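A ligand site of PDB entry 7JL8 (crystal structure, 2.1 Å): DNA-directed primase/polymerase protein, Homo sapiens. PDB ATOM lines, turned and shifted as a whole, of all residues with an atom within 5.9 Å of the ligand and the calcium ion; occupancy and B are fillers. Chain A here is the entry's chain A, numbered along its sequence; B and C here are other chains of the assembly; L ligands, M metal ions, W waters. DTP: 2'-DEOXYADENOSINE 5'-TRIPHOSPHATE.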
ATOM      1  N   GLY A  74     -12.177 -25.133  11.548  1.00  0.00           N
ATOM      2  CA  GLY A  74     -12.459 -25.598  12.884  1.00  0.00           C
ATOM      3  C   GLY A  74     -13.910 -25.459  13.287  1.00  0.00           C
ATOM      4  O   GLY A  74     -14.217 -25.466  14.493  1.00  0.00           O
ATOM      5  N   ARG A  76     -17.573 -26.320  14.354  1.00  0.00           N
ATOM      6  CA  ARG A  76     -17.978 -27.378  15.277  1.00  0.00           C
ATOM      7  C   ARG A  76     -19.481 -27.276  15.484  1.00  0.00           C
ATOM      8  O   ARG A  76     -20.074 -26.213  15.397  1.00  0.00           O
ATOM      9  CB  ARG A  76     -17.229 -27.265  16.615  1.00  0.00           C
ATOM     10  CG  ARG A  76     -15.750 -27.570  16.439  1.00  0.00           C
ATOM     11  CD  ARG A  76     -14.850 -27.035  17.541  1.00  0.00           C
ATOM     12  NE  ARG A  76     -13.478 -27.018  17.025  1.00  0.00           N
ATOM     13  CZ  ARG A  76     -12.567 -27.959  17.232  1.00  0.00           C
ATOM     14  NH1 ARG A  76     -12.864 -28.985  17.992  1.00  0.00           N
ATOM     15  NH2 ARG A  76     -11.365 -27.888  16.698  1.00  0.00           N
ATOM     16  N   TYR A 100     -14.734 -33.995  20.452  1.00  0.00           N
ATOM     17  CA  TYR A 100     -14.049 -33.259  21.502  1.00  0.00           C
ATOM     18  C   TYR A 100     -14.968 -33.153  22.707  1.00  0.00           C
ATOM     19  O   TYR A 100     -16.191 -33.089  22.575  1.00  0.00           O
ATOM     20  CB  TYR A 100     -13.621 -31.854  20.992  1.00  0.00           C
ATOM     21  CG  TYR A 100     -12.670 -31.923  19.812  1.00  0.00           C
ATOM     22  CD1 TYR A 100     -13.138 -32.245  18.542  1.00  0.00           C
ATOM     23  CD2 TYR A 100     -11.306 -31.697  19.974  1.00  0.00           C
ATOM     24  CE1 TYR A 100     -12.255 -32.339  17.453  1.00  0.00           C
ATOM     25  CE2 TYR A 100     -10.428 -31.776  18.899  1.00  0.00           C
ATOM     26  CZ  TYR A 100     -10.910 -32.096  17.649  1.00  0.00           C
ATOM     27  OH  TYR A 100     -10.026 -32.180  16.595  1.00  0.00           O
ATOM     28  N   ASP A 114      -1.647 -30.982  28.012  1.00  0.00           N
ATOM     29  CA  ASP A 114      -1.420 -31.183  26.588  1.00  0.00           C
ATOM     30  C   ASP A 114       0.083 -31.006  26.330  1.00  0.00           C
ATOM     31  O   ASP A 114       0.634 -29.937  26.580  1.00  0.00           O
ATOM     32  CB  ASP A 114      -2.241 -30.213  25.755  1.00  0.00           C
ATOM     33  CG  ASP A 114      -2.101 -30.453  24.264  1.00  0.00           C
ATOM     34  OD1 ASP A 114      -2.502 -31.532  23.789  1.00  0.00           O
ATOM     35  OD2 ASP A 114      -1.663 -29.543  23.543  1.00  0.00           O
ATOM     36  N   LEU A 115       0.739 -32.075  25.877  1.00  0.00           N
ATOM     37  CA  LEU A 115       2.179 -32.125  25.760  1.00  0.00           C
ATOM     38  C   LEU A 115       2.551 -32.390  24.310  1.00  0.00           C
ATOM     39  O   LEU A 115       1.950 -33.250  23.658  1.00  0.00           O
ATOM     40  CB  LEU A 115       2.774 -33.230  26.668  1.00  0.00           C
ATOM     41  CG  LEU A 115       2.393 -33.153  28.158  1.00  0.00           C
ATOM     42  CD1 LEU A 115       3.015 -34.330  28.899  1.00  0.00           C
ATOM     43  CD2 LEU A 115       2.837 -31.834  28.794  1.00  0.00           C
ATOM     44  N   GLU A 116       3.537 -31.649  23.800  1.00  0.00           N
ATOM     45  CA  GLU A 116       3.873 -31.655  22.386  1.00  0.00           C
ATOM     46  C   GLU A 116       5.301 -31.149  22.194  1.00  0.00           C
ATOM     47  O   GLU A 116       5.746 -30.257  22.914  1.00  0.00           O
ATOM     48  CB  GLU A 116       2.968 -30.731  21.561  1.00  0.00           C
ATOM     49  CG  GLU A 116       1.510 -31.010  21.649  1.00  0.00           C
ATOM     50  CD  GLU A 116       0.701 -29.928  20.967  1.00  0.00           C
ATOM     51  OE1 GLU A 116       0.963 -28.736  21.210  1.00  0.00           O
ATOM     52  OE2 GLU A 116      -0.198 -30.273  20.169  1.00  0.00           O
ATOM     53  N   SER A 160      -1.000 -39.513  20.837  1.00  0.00           N
ATOM     54  CA  SER A 160      -1.430 -39.240  19.472  1.00  0.00           C
ATOM     55  C   SER A 160      -0.234 -38.858  18.590  1.00  0.00           C
ATOM     56  O   SER A 160      -0.370 -38.054  17.664  1.00  0.00           O
ATOM     57  CB  SER A 160      -2.486 -38.130  19.439  1.00  0.00           C
ATOM     58  OG  SER A 160      -3.102 -38.064  18.156  1.00  0.00           O
ATOM     59  N   SER A 161       0.930 -39.447  18.869  1.00  0.00           N
ATOM     60  CA  SER A 161       2.171 -39.069  18.202  1.00  0.00           C
ATOM     61  C   SER A 161       2.194 -39.495  16.741  1.00  0.00           C
ATOM     62  O   SER A 161       1.617 -40.517  16.361  1.00  0.00           O
ATOM     63  CB  SER A 161       3.358 -39.698  18.931  1.00  0.00           C
ATOM     64  OG  SER A 161       3.556 -39.133  20.201  1.00  0.00           O
ATOM     65  N   LYS A 165       5.485 -35.442  15.080  1.00  0.00           N
ATOM     66  CA  LYS A 165       5.054 -34.804  16.305  1.00  0.00           C
ATOM     67  C   LYS A 165       4.963 -35.809  17.451  1.00  0.00           C
ATOM     68  O   LYS A 165       4.296 -36.835  17.324  1.00  0.00           O
ATOM     69  CB  LYS A 165       3.694 -34.122  16.118  1.00  0.00           C
ATOM     70  CG  LYS A 165       3.301 -33.249  17.283  1.00  0.00           C
ATOM     71  CD  LYS A 165       2.063 -32.427  16.957  1.00  0.00           C
ATOM     72  CE  LYS A 165       1.681 -31.498  18.115  1.00  0.00           C
ATOM     73  NZ  LYS A 165       0.561 -30.571  17.744  1.00  0.00           N
ATOM     74  N   SER A 167       3.157 -36.276  20.734  1.00  0.00           N
ATOM     75  CA  SER A 167       1.907 -35.703  21.226  1.00  0.00           C
ATOM     76  C   SER A 167       1.322 -36.599  22.313  1.00  0.00           C
ATOM     77  O   SER A 167       1.061 -37.776  22.068  1.00  0.00           O
ATOM     78  CB  SER A 167       0.905 -35.551  20.067  1.00  0.00           C
ATOM     79  OG  SER A 167      -0.351 -35.080  20.525  1.00  0.00           O
ATOM     80  N   ARG A 168       1.107 -36.041  23.505  1.00  0.00           N
ATOM     81  CA  ARG A 168       0.503 -36.779  24.600  1.00  0.00           C
ATOM     82  C   ARG A 168      -0.588 -35.949  25.253  1.00  0.00           C
ATOM     83  O   ARG A 168      -0.555 -34.717  25.223  1.00  0.00           O
ATOM     84  CB  ARG A 168       1.540 -37.202  25.687  1.00  0.00           C
ATOM     85  CG  ARG A 168       2.686 -38.084  25.192  1.00  0.00           C
ATOM     86  CD  ARG A 168       2.354 -39.544  25.178  1.00  0.00           C
ATOM     87  NE  ARG A 168       3.471 -40.359  24.641  1.00  0.00           N
ATOM     88  CZ  ARG A 168       4.381 -40.984  25.390  1.00  0.00           C
ATOM     89  NH1 ARG A 168       4.363 -40.931  26.738  1.00  0.00           N
ATOM     90  NH2 ARG A 168       5.342 -41.665  24.767  1.00  0.00           N
ATOM     91  N   HIS A 169      -1.559 -36.648  25.837  1.00  0.00           N
ATOM     92  CA  HIS A 169      -2.529 -36.054  26.752  1.00  0.00           C
ATOM     93  C   HIS A 169      -2.399 -36.819  28.056  1.00  0.00           C
ATOM     94  O   HIS A 169      -2.464 -38.053  28.051  1.00  0.00           O
ATOM     95  CB  HIS A 169      -3.957 -36.167  26.230  1.00  0.00           C
ATOM     96  CG  HIS A 169      -4.282 -35.193  25.136  1.00  0.00           C
ATOM     97  ND1 HIS A 169      -5.559 -35.031  24.643  1.00  0.00           N
ATOM     98  CD2 HIS A 169      -3.488 -34.350  24.427  1.00  0.00           C
ATOM     99  CE1 HIS A 169      -5.533 -34.128  23.681  1.00  0.00           C
ATOM    100  NE2 HIS A 169      -4.294 -33.691  23.531  1.00  0.00           N
ATOM    101  N   ASP A 280       1.787 -27.390  26.899  1.00  0.00           N
ATOM    102  CA  ASP A 280       0.979 -26.435  26.145  1.00  0.00           C
ATOM    103  C   ASP A 280       0.021 -25.745  27.116  1.00  0.00           C
ATOM    104  O   ASP A 280      -0.948 -26.355  27.588  1.00  0.00           O
ATOM    105  CB  ASP A 280       0.241 -27.168  25.028  1.00  0.00           C
ATOM    106  CG  ASP A 280      -0.712 -26.288  24.259  1.00  0.00           C
ATOM    107  OD1 ASP A 280      -0.754 -25.048  24.460  1.00  0.00           O
ATOM    108  OD2 ASP A 280      -1.436 -26.869  23.424  1.00  0.00           O
ATOM    109  N   VAL A 283      -4.429 -24.637  26.594  1.00  0.00           N
ATOM    110  CA  VAL A 283      -5.614 -25.469  26.719  1.00  0.00           C
ATOM    111  C   VAL A 283      -6.390 -25.176  28.013  1.00  0.00           C
ATOM    112  O   VAL A 283      -7.365 -25.856  28.313  1.00  0.00           O
ATOM    113  CB  VAL A 283      -5.249 -26.965  26.629  1.00  0.00           C
ATOM    114  CG1 VAL A 283      -4.594 -27.259  25.284  1.00  0.00           C
ATOM    115  CG2 VAL A 283      -4.360 -27.392  27.778  1.00  0.00           C
ATOM    116  N   ARG A 288     -12.684 -24.862  26.810  1.00  0.00           N
ATOM    117  CA  ARG A 288     -11.700 -25.534  25.986  1.00  0.00           C
ATOM    118  C   ARG A 288     -12.223 -26.893  25.511  1.00  0.00           C
ATOM    119  O   ARG A 288     -12.706 -27.717  26.306  1.00  0.00           O
ATOM    120  CB  ARG A 288     -10.404 -25.720  26.780  1.00  0.00           C
ATOM    121  CG  ARG A 288      -9.390 -26.656  26.107  1.00  0.00           C
ATOM    122  CD  ARG A 288      -8.915 -26.116  24.734  1.00  0.00           C
ATOM    123  NE  ARG A 288      -8.682 -24.681  24.737  1.00  0.00           N
ATOM    124  CZ  ARG A 288      -8.164 -24.013  23.712  1.00  0.00           C
ATOM    125  NH1 ARG A 288      -7.802 -24.646  22.604  1.00  0.00           N
ATOM    126  NH2 ARG A 288      -8.009 -22.711  23.794  1.00  0.00           N
ATOM    127  N   ASN A 289     -12.126 -27.101  24.210  1.00  0.00           N
ATOM    128  CA  ASN A 289     -12.321 -28.411  23.598  1.00  0.00           C
ATOM    129  C   ASN A 289     -11.066 -29.253  23.779  1.00  0.00           C
ATOM    130  O   ASN A 289      -9.947 -28.747  23.639  1.00  0.00           O
ATOM    131  CB  ASN A 289     -12.601 -28.276  22.100  1.00  0.00           C
ATOM    132  CG  ASN A 289     -13.880 -27.523  21.792  1.00  0.00           C
ATOM    133  OD1 ASN A 289     -14.305 -26.655  22.552  1.00  0.00           O
ATOM    134  ND2 ASN A 289     -14.505 -27.867  20.693  1.00  0.00           N
ATOM    135  N   PHE A 290     -11.250 -30.532  24.106  1.00  0.00           N
ATOM    136  CA  PHE A 290     -10.140 -31.440  24.374  1.00  0.00           C
ATOM    137  C   PHE A 290     -10.449 -32.773  23.703  1.00  0.00           C
ATOM    138  O   PHE A 290     -11.351 -33.501  24.148  1.00  0.00           O
ATOM    139  CB  PHE A 290      -9.913 -31.602  25.876  1.00  0.00           C
ATOM    140  CG  PHE A 290      -8.495 -31.935  26.249  1.00  0.00           C
ATOM    141  CD1 PHE A 290      -7.436 -31.140  25.824  1.00  0.00           C
ATOM    142  CD2 PHE A 290      -8.212 -33.024  27.060  1.00  0.00           C
ATOM    143  CE1 PHE A 290      -6.127 -31.436  26.176  1.00  0.00           C
ATOM    144  CE2 PHE A 290      -6.906 -33.325  27.437  1.00  0.00           C
ATOM    145  CZ  PHE A 290      -5.856 -32.532  26.985  1.00  0.00           C
ATOM    146  N   ARG A 291      -9.666 -33.114  22.679  1.00  0.00           N
ATOM    147  CA  ARG A 291      -9.979 -34.258  21.824  1.00  0.00           C
ATOM    148  C   ARG A 291     -10.184 -35.514  22.654  1.00  0.00           C
ATOM    149  O   ARG A 291      -9.446 -35.791  23.594  1.00  0.00           O
ATOM    150  CB  ARG A 291      -8.860 -34.460  20.809  1.00  0.00           C
ATOM    151  CG  ARG A 291      -9.150 -35.534  19.778  1.00  0.00           C
ATOM    152  CD  ARG A 291      -8.343 -35.323  18.489  1.00  0.00           C
ATOM    153  NE  ARG A 291      -6.918 -35.116  18.714  1.00  0.00           N
ATOM    154  CZ  ARG A 291      -5.964 -36.034  18.549  1.00  0.00           C
ATOM    155  NH1 ARG A 291      -6.268 -37.271  18.182  1.00  0.00           N
ATOM    156  NH2 ARG A 291      -4.686 -35.710  18.753  1.00  0.00           N
ATOM    157  N   LYS A 297      -7.989 -35.782  14.798  1.00  0.00           N
ATOM    158  CA  LYS A 297      -8.306 -34.531  14.112  1.00  0.00           C
ATOM    159  C   LYS A 297      -8.873 -34.846  12.723  1.00  0.00           C
ATOM    160  O   LYS A 297      -8.528 -35.855  12.104  1.00  0.00           O
ATOM    161  CB  LYS A 297      -7.078 -33.642  14.013  1.00  0.00           C
ATOM    162  CG  LYS A 297      -6.674 -33.017  15.324  1.00  0.00           C
ATOM    163  CD  LYS A 297      -5.381 -32.219  15.182  1.00  0.00           C
ATOM    164  CE  LYS A 297      -5.319 -31.084  16.176  1.00  0.00           C
ATOM    165  NZ  LYS A 297      -3.995 -30.437  16.192  1.00  0.00           N
ATOM    166  N   VAL A 302      -4.520 -40.296  13.087  1.00  0.00           N
ATOM    167  CA  VAL A 302      -4.010 -40.755  14.373  1.00  0.00           C
ATOM    168  C   VAL A 302      -4.998 -40.386  15.475  1.00  0.00           C
ATOM    169  O   VAL A 302      -5.282 -39.213  15.721  1.00  0.00           O
ATOM    170  CB  VAL A 302      -2.611 -40.166  14.645  1.00  0.00           C
ATOM    171  CG1 VAL A 302      -2.647 -38.643  14.674  1.00  0.00           C
ATOM    172  CG2 VAL A 302      -2.065 -40.730  15.965  1.00  0.00           C
ATOM    173  N   LEU A 304      -6.211 -40.673  19.583  1.00  0.00           N
ATOM    174  CA  LEU A 304      -5.664 -40.809  20.930  1.00  0.00           C
ATOM    175  C   LEU A 304      -5.931 -42.221  21.419  1.00  0.00           C
ATOM    176  O   LEU A 304      -7.061 -42.715  21.353  1.00  0.00           O
ATOM    177  CB  LEU A 304      -6.253 -39.757  21.869  1.00  0.00           C
ATOM    178  CG  LEU A 304      -5.656 -38.350  21.699  1.00  0.00           C
ATOM    179  CD1 LEU A 304      -6.673 -37.272  22.035  1.00  0.00           C
ATOM    180  CD2 LEU A 304      -4.405 -38.154  22.545  1.00  0.00           C
ATOM    181  P    DT B   3     -19.260 -20.748  12.389  1.00  0.00           P
ATOM    182  OP1  DT B   3     -18.640 -19.407  12.440  1.00  0.00           O
ATOM    183  OP2  DT B   3     -19.079 -21.615  11.215  1.00  0.00           O
ATOM    184  O5'  DT B   3     -18.719 -21.559  13.640  1.00  0.00           O
ATOM    185  C5'  DT B   3     -19.412 -22.718  14.096  1.00  0.00           C
ATOM    186  C4'  DT B   3     -18.993 -23.033  15.534  1.00  0.00           C
ATOM    187  O4'  DT B   3     -17.650 -23.525  15.527  1.00  0.00           O
ATOM    188  C3'  DT B   3     -19.023 -21.824  16.455  1.00  0.00           C
ATOM    189  O3'  DT B   3     -19.947 -22.055  17.538  1.00  0.00           O
ATOM    190  C2'  DT B   3     -17.574 -21.638  16.928  1.00  0.00           C
ATOM    191  C1'  DT B   3     -16.926 -22.966  16.601  1.00  0.00           C
ATOM    192  N1   DT B   3     -15.499 -22.871  16.180  1.00  0.00           N
ATOM    193  C2   DT B   3     -14.504 -23.254  17.055  1.00  0.00           C
ATOM    194  O2   DT B   3     -14.716 -23.669  18.172  1.00  0.00           O
ATOM    195  N3   DT B   3     -13.234 -23.131  16.562  1.00  0.00           N
ATOM    196  C4   DT B   3     -12.875 -22.677  15.306  1.00  0.00           C
ATOM    197  O4   DT B   3     -11.710 -22.596  14.954  1.00  0.00           O
ATOM    198  C5   DT B   3     -13.962 -22.297  14.438  1.00  0.00           C
ATOM    199  C7   DT B   3     -13.676 -21.793  13.068  1.00  0.00           C
ATOM    200  C6   DT B   3     -15.207 -22.408  14.907  1.00  0.00           C
ATOM    201  P   8OG B   4     -20.117 -20.962  18.706  1.00  0.00           P
ATOM    202  OP1 8OG B   4     -21.463 -21.069  19.422  1.00  0.00           O
ATOM    203  OP2 8OG B   4     -19.915 -19.596  18.151  1.00  0.00           O
ATOM    204  O5' 8OG B   4     -18.930 -21.321  19.756  1.00  0.00           O
ATOM    205  C5' 8OG B   4     -18.519 -20.284  20.573  1.00  0.00           C
ATOM    206  C4' 8OG B   4     -17.177 -20.650  21.113  1.00  0.00           C
ATOM    207  O4' 8OG B   4     -16.122 -21.037  19.992  1.00  0.00           O
ATOM    208  C3' 8OG B   4     -16.701 -19.590  21.730  1.00  0.00           C
ATOM    209  O3' 8OG B   4     -16.678 -19.926  23.183  1.00  0.00           O
ATOM    210  C2' 8OG B   4     -15.317 -19.318  21.205  1.00  0.00           C
ATOM    211  C1' 8OG B   4     -14.979 -20.595  20.445  1.00  0.00           C
ATOM    212  N9  8OG B   4     -14.070 -20.343  19.342  1.00  0.00           N
ATOM    213  C8  8OG B   4     -14.379 -19.635  18.048  1.00  0.00           C
ATOM    214  N7  8OG B   4     -13.095 -19.691  17.230  1.00  0.00           N
ATOM    215  C5  8OG B   4     -12.109 -20.399  18.036  1.00  0.00           C
ATOM    216  C6  8OG B   4     -10.669 -20.741  17.740  1.00  0.00           C
ATOM    217  O6  8OG B   4     -10.158 -20.440  16.731  1.00  0.00           O
ATOM    218  N1  8OG B   4      -9.905 -21.463  18.714  1.00  0.00           N
ATOM    219  C2  8OG B   4     -10.535 -21.857  19.999  1.00  0.00           C
ATOM    220  N2  8OG B   4      -9.769 -22.571  20.979  1.00  0.00           N
ATOM    221  N3  8OG B   4     -11.895 -21.518  20.284  1.00  0.00           N
ATOM    222  C4  8OG B   4     -12.690 -20.784  19.275  1.00  0.00           C
ATOM    223  O8  8OG B   4     -15.438 -19.130  17.749  1.00  0.00           O
ATOM    224  P    DC C  13      -0.366 -24.164  17.824  1.00  0.00           P
ATOM    225  OP1  DC C  13       0.940 -24.717  18.249  1.00  0.00           O
ATOM    226  OP2  DC C  13      -0.918 -24.496  16.484  1.00  0.00           O
ATOM    227  O5'  DC C  13      -1.455 -24.536  18.947  1.00  0.00           O
ATOM    228  C5'  DC C  13      -1.232 -24.178  20.299  1.00  0.00           C
ATOM    229  C4'  DC C  13      -2.557 -24.063  21.044  1.00  0.00           C
ATOM    230  O4'  DC C  13      -3.462 -23.248  20.271  1.00  0.00           O
ATOM    231  C3'  DC C  13      -3.296 -25.389  21.282  1.00  0.00           C
ATOM    232  O3'  DC C  13      -3.483 -25.566  22.700  1.00  0.00           O
ATOM    233  C2'  DC C  13      -4.626 -25.276  20.526  1.00  0.00           C
ATOM    234  C1'  DC C  13      -4.779 -23.764  20.385  1.00  0.00           C
ATOM    235  N1   DC C  13      -5.545 -23.328  19.226  1.00  0.00           N
ATOM    236  C2   DC C  13      -6.875 -22.944  19.394  1.00  0.00           C
ATOM    237  O2   DC C  13      -7.358 -23.001  20.517  1.00  0.00           O
ATOM    238  N3   DC C  13      -7.583 -22.531  18.322  1.00  0.00           N
ATOM    239  C4   DC C  13      -6.999 -22.469  17.121  1.00  0.00           C
ATOM    240  N4   DC C  13      -7.746 -22.037  16.090  1.00  0.00           N
ATOM    241  C5   DC C  13      -5.644 -22.842  16.930  1.00  0.00           C
ATOM    242  C6   DC C  13      -4.957 -23.261  18.001  1.00  0.00           C
HETATM  243  PG  DTP L   1      -2.241 -32.956  18.432  1.00  0.00           P
HETATM  244  O1G DTP L   1      -2.264 -32.418  17.008  1.00  0.00           O
HETATM  245  O2G DTP L   1      -1.419 -32.093  19.356  1.00  0.00           O
HETATM  246  O3G DTP L   1      -1.837 -34.400  18.556  1.00  0.00           O
HETATM  247  PB  DTP L   1      -4.571 -32.062  20.007  1.00  0.00           P
HETATM  248  O1B DTP L   1      -5.983 -32.555  20.015  1.00  0.00           O
HETATM  249  O2B DTP L   1      -3.676 -32.108  21.207  1.00  0.00           O
HETATM  250  O3B DTP L   1      -3.828 -32.906  18.818  1.00  0.00           O
HETATM  251  PA  DTP L   1      -3.916 -29.195  19.745  1.00  0.00           P
HETATM  252  O1A DTP L   1      -3.769 -28.437  18.459  1.00  0.00           O
HETATM  253  O2A DTP L   1      -2.691 -29.490  20.570  1.00  0.00           O
HETATM  254  O3A DTP L   1      -4.731 -30.563  19.378  1.00  0.00           O
HETATM  255  O5' DTP L   1      -5.007 -28.368  20.600  1.00  0.00           O
HETATM  256  C5' DTP L   1      -5.368 -28.834  21.887  1.00  0.00           C
HETATM  257  C4' DTP L   1      -6.867 -28.883  22.000  1.00  0.00           C
HETATM  258  O4' DTP L   1      -7.425 -27.591  21.780  1.00  0.00           O
HETATM  259  C3' DTP L   1      -7.560 -29.799  20.995  1.00  0.00           C
HETATM  260  O3' DTP L   1      -7.751 -31.135  21.410  1.00  0.00           O
HETATM  261  C2' DTP L   1      -8.924 -29.136  20.766  1.00  0.00           C
HETATM  262  C1' DTP L   1      -8.687 -27.665  21.114  1.00  0.00           C
HETATM  263  N9  DTP L   1      -8.623 -26.939  19.834  1.00  0.00           N
HETATM  264  C8  DTP L   1      -7.561 -26.953  19.001  1.00  0.00           C
HETATM  265  N7  DTP L   1      -7.798 -26.210  17.897  1.00  0.00           N
HETATM  266  C5  DTP L   1      -9.043 -25.720  18.015  1.00  0.00           C
HETATM  267  C6  DTP L   1      -9.906 -24.860  17.203  1.00  0.00           C
HETATM  268  N6  DTP L   1      -9.428 -24.395  16.021  1.00  0.00           N
HETATM  269  N1  DTP L   1     -11.141 -24.567  17.661  1.00  0.00           N
HETATM  270  C2  DTP L   1     -11.579 -25.041  18.839  1.00  0.00           C
HETATM  271  N3  DTP L   1     -10.824 -25.821  19.626  1.00  0.00           N
HETATM  272  C4  DTP L   1      -9.588 -26.195  19.287  1.00  0.00           C
HETATM  273 CA    CA M   1      -1.574 -31.094  21.566  1.00  0.00          CA
HETATM  274  O   HOH W   1      -0.405 -33.110  22.265  1.00  0.00           O
HETATM  275  O   HOH W   2     -11.162 -25.068  22.539  1.00  0.00           O
HETATM  276  O   HOH W   3      -9.047 -29.467  17.134  1.00  0.00           O
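An oxygen (O3G) of the ligand lies within hydrogen-bond range of the side-chain hydroxyl of Ser 167, at 2.6 Å.
NZ of Lys 297 is in salt-bridge range of O1G of the ligand (2.8 Å).
O4 of DT 3 of chain B lies within hydrogen-bond range of N6 of the ligand, at 3.1 Å.
NE2 of His 169 sits close to O2B of the ligand, 2.9 Å away.
N4 of DC 13 of chain C is in hydrogen-bond range of a nitrogen (N6) of the ligand, 2.9 Å away.
O3' of the ligand lies within hydrogen-bond range of N of Arg 291 (3.0 Å).
O1B of the ligand is in salt-bridge range of NE of Arg 291 (3.0 Å).
The side-chain amino group (NZ) of Lys 165 lies within salt-bridge range of an oxygen (O1G) of the ligand (3.5 Å).
The guanidinium group of Arg 288 lies within hydrogen-bond range of an oxygen (O4') of the ligand (3.1 Å).
The guanidinium group of Arg 76 sits close to a nitrogen (N1) of the ligand (3.4 Å).
The side-chain carboxylate (OE1) of Glu 116 lies within salt-bridge range of the side-chain amino group (NZ) of Lys 165.
NE2 of His 169 lies close to OD1 of Asp 114 (2.8 Å).
The backbone carbonyl oxygen (O) of Asp 114 is in hydrogen-bond range of the backbone NH (N) of Asp 280 (2.8 Å).
N of Arg 76 sits at hydrogen-bond distance from O4' of DT 3 of chain B, at 3.0 Å.
O2 of DC 13 of chain C is in hydrogen-bond range of the guanidinium group (NH1) of Arg 288, 2.7 Å away.
ND2 of Asn 289 sits close to NH1 of Arg 76 (3.4 Å).
The guanidinium group (NE) of Arg 76 lies within hydrogen-bond range of the backbone carbonyl oxygen (O) of Gly 74, at 3.1 Å.
OG of Ser 160 sits at hydrogen-bond distance from O of Val 302, 3.5 Å away.
O of Asn 289 sits close to O4' of the ligand (3.3 Å).
CE2 of Tyr 100 touches C2' of the ligand, at 3.6 Å.
Ser 160 touches the ligand.
Val 283 touches the ligand (CG1 to C5', 3.8 Å).
Phe 290 touches the ligand.
8OG 4 of chain B touches the ligand.
Hydrophobic or aromatic side chains within 4 Å of the ligand: Tyr 100, His 169 and Val 283.
Of the 24 residues printed, 17 come within 4 Å of the ligand.
Two residues have an atom within 4 Å of the calcium ion: Asp 114 and Glu 116.
The side-chain carboxylate (OE2) of Glu 116 binds the calcium ion, at 2.1 Å.
An oxygen (O2A) of the ligand is bound to the calcium ion (2.2 Å).
O2B of the ligand is bound to the calcium ion, 2.4 Å away.
The calcium ion is bound by O2G of the ligand (2.4 Å).
Water W1 is bound to the calcium ion (2.4 Å).
The calcium ion is bound by OD1 of Asp 114 (2.4 Å).
OD2 of Asp 114 binds the calcium ion.
Water W1 lies within hydrogen-bond range of OG of Ser 167 (2.6 Å), O of Leu 115 (2.7 Å) and O of Arg 168 (3.4 Å).
Water W2 lies within hydrogen-bond range of the backbone NH of Asn 289, a nitrogen (N3) of the ligand, N2 of 8OG 4 of chain B and the guanidinium group of Arg 288.
Water W3 bridges NH2 of Arg 76 (2.8 Å) and OH of Tyr 100 (2.9 Å).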
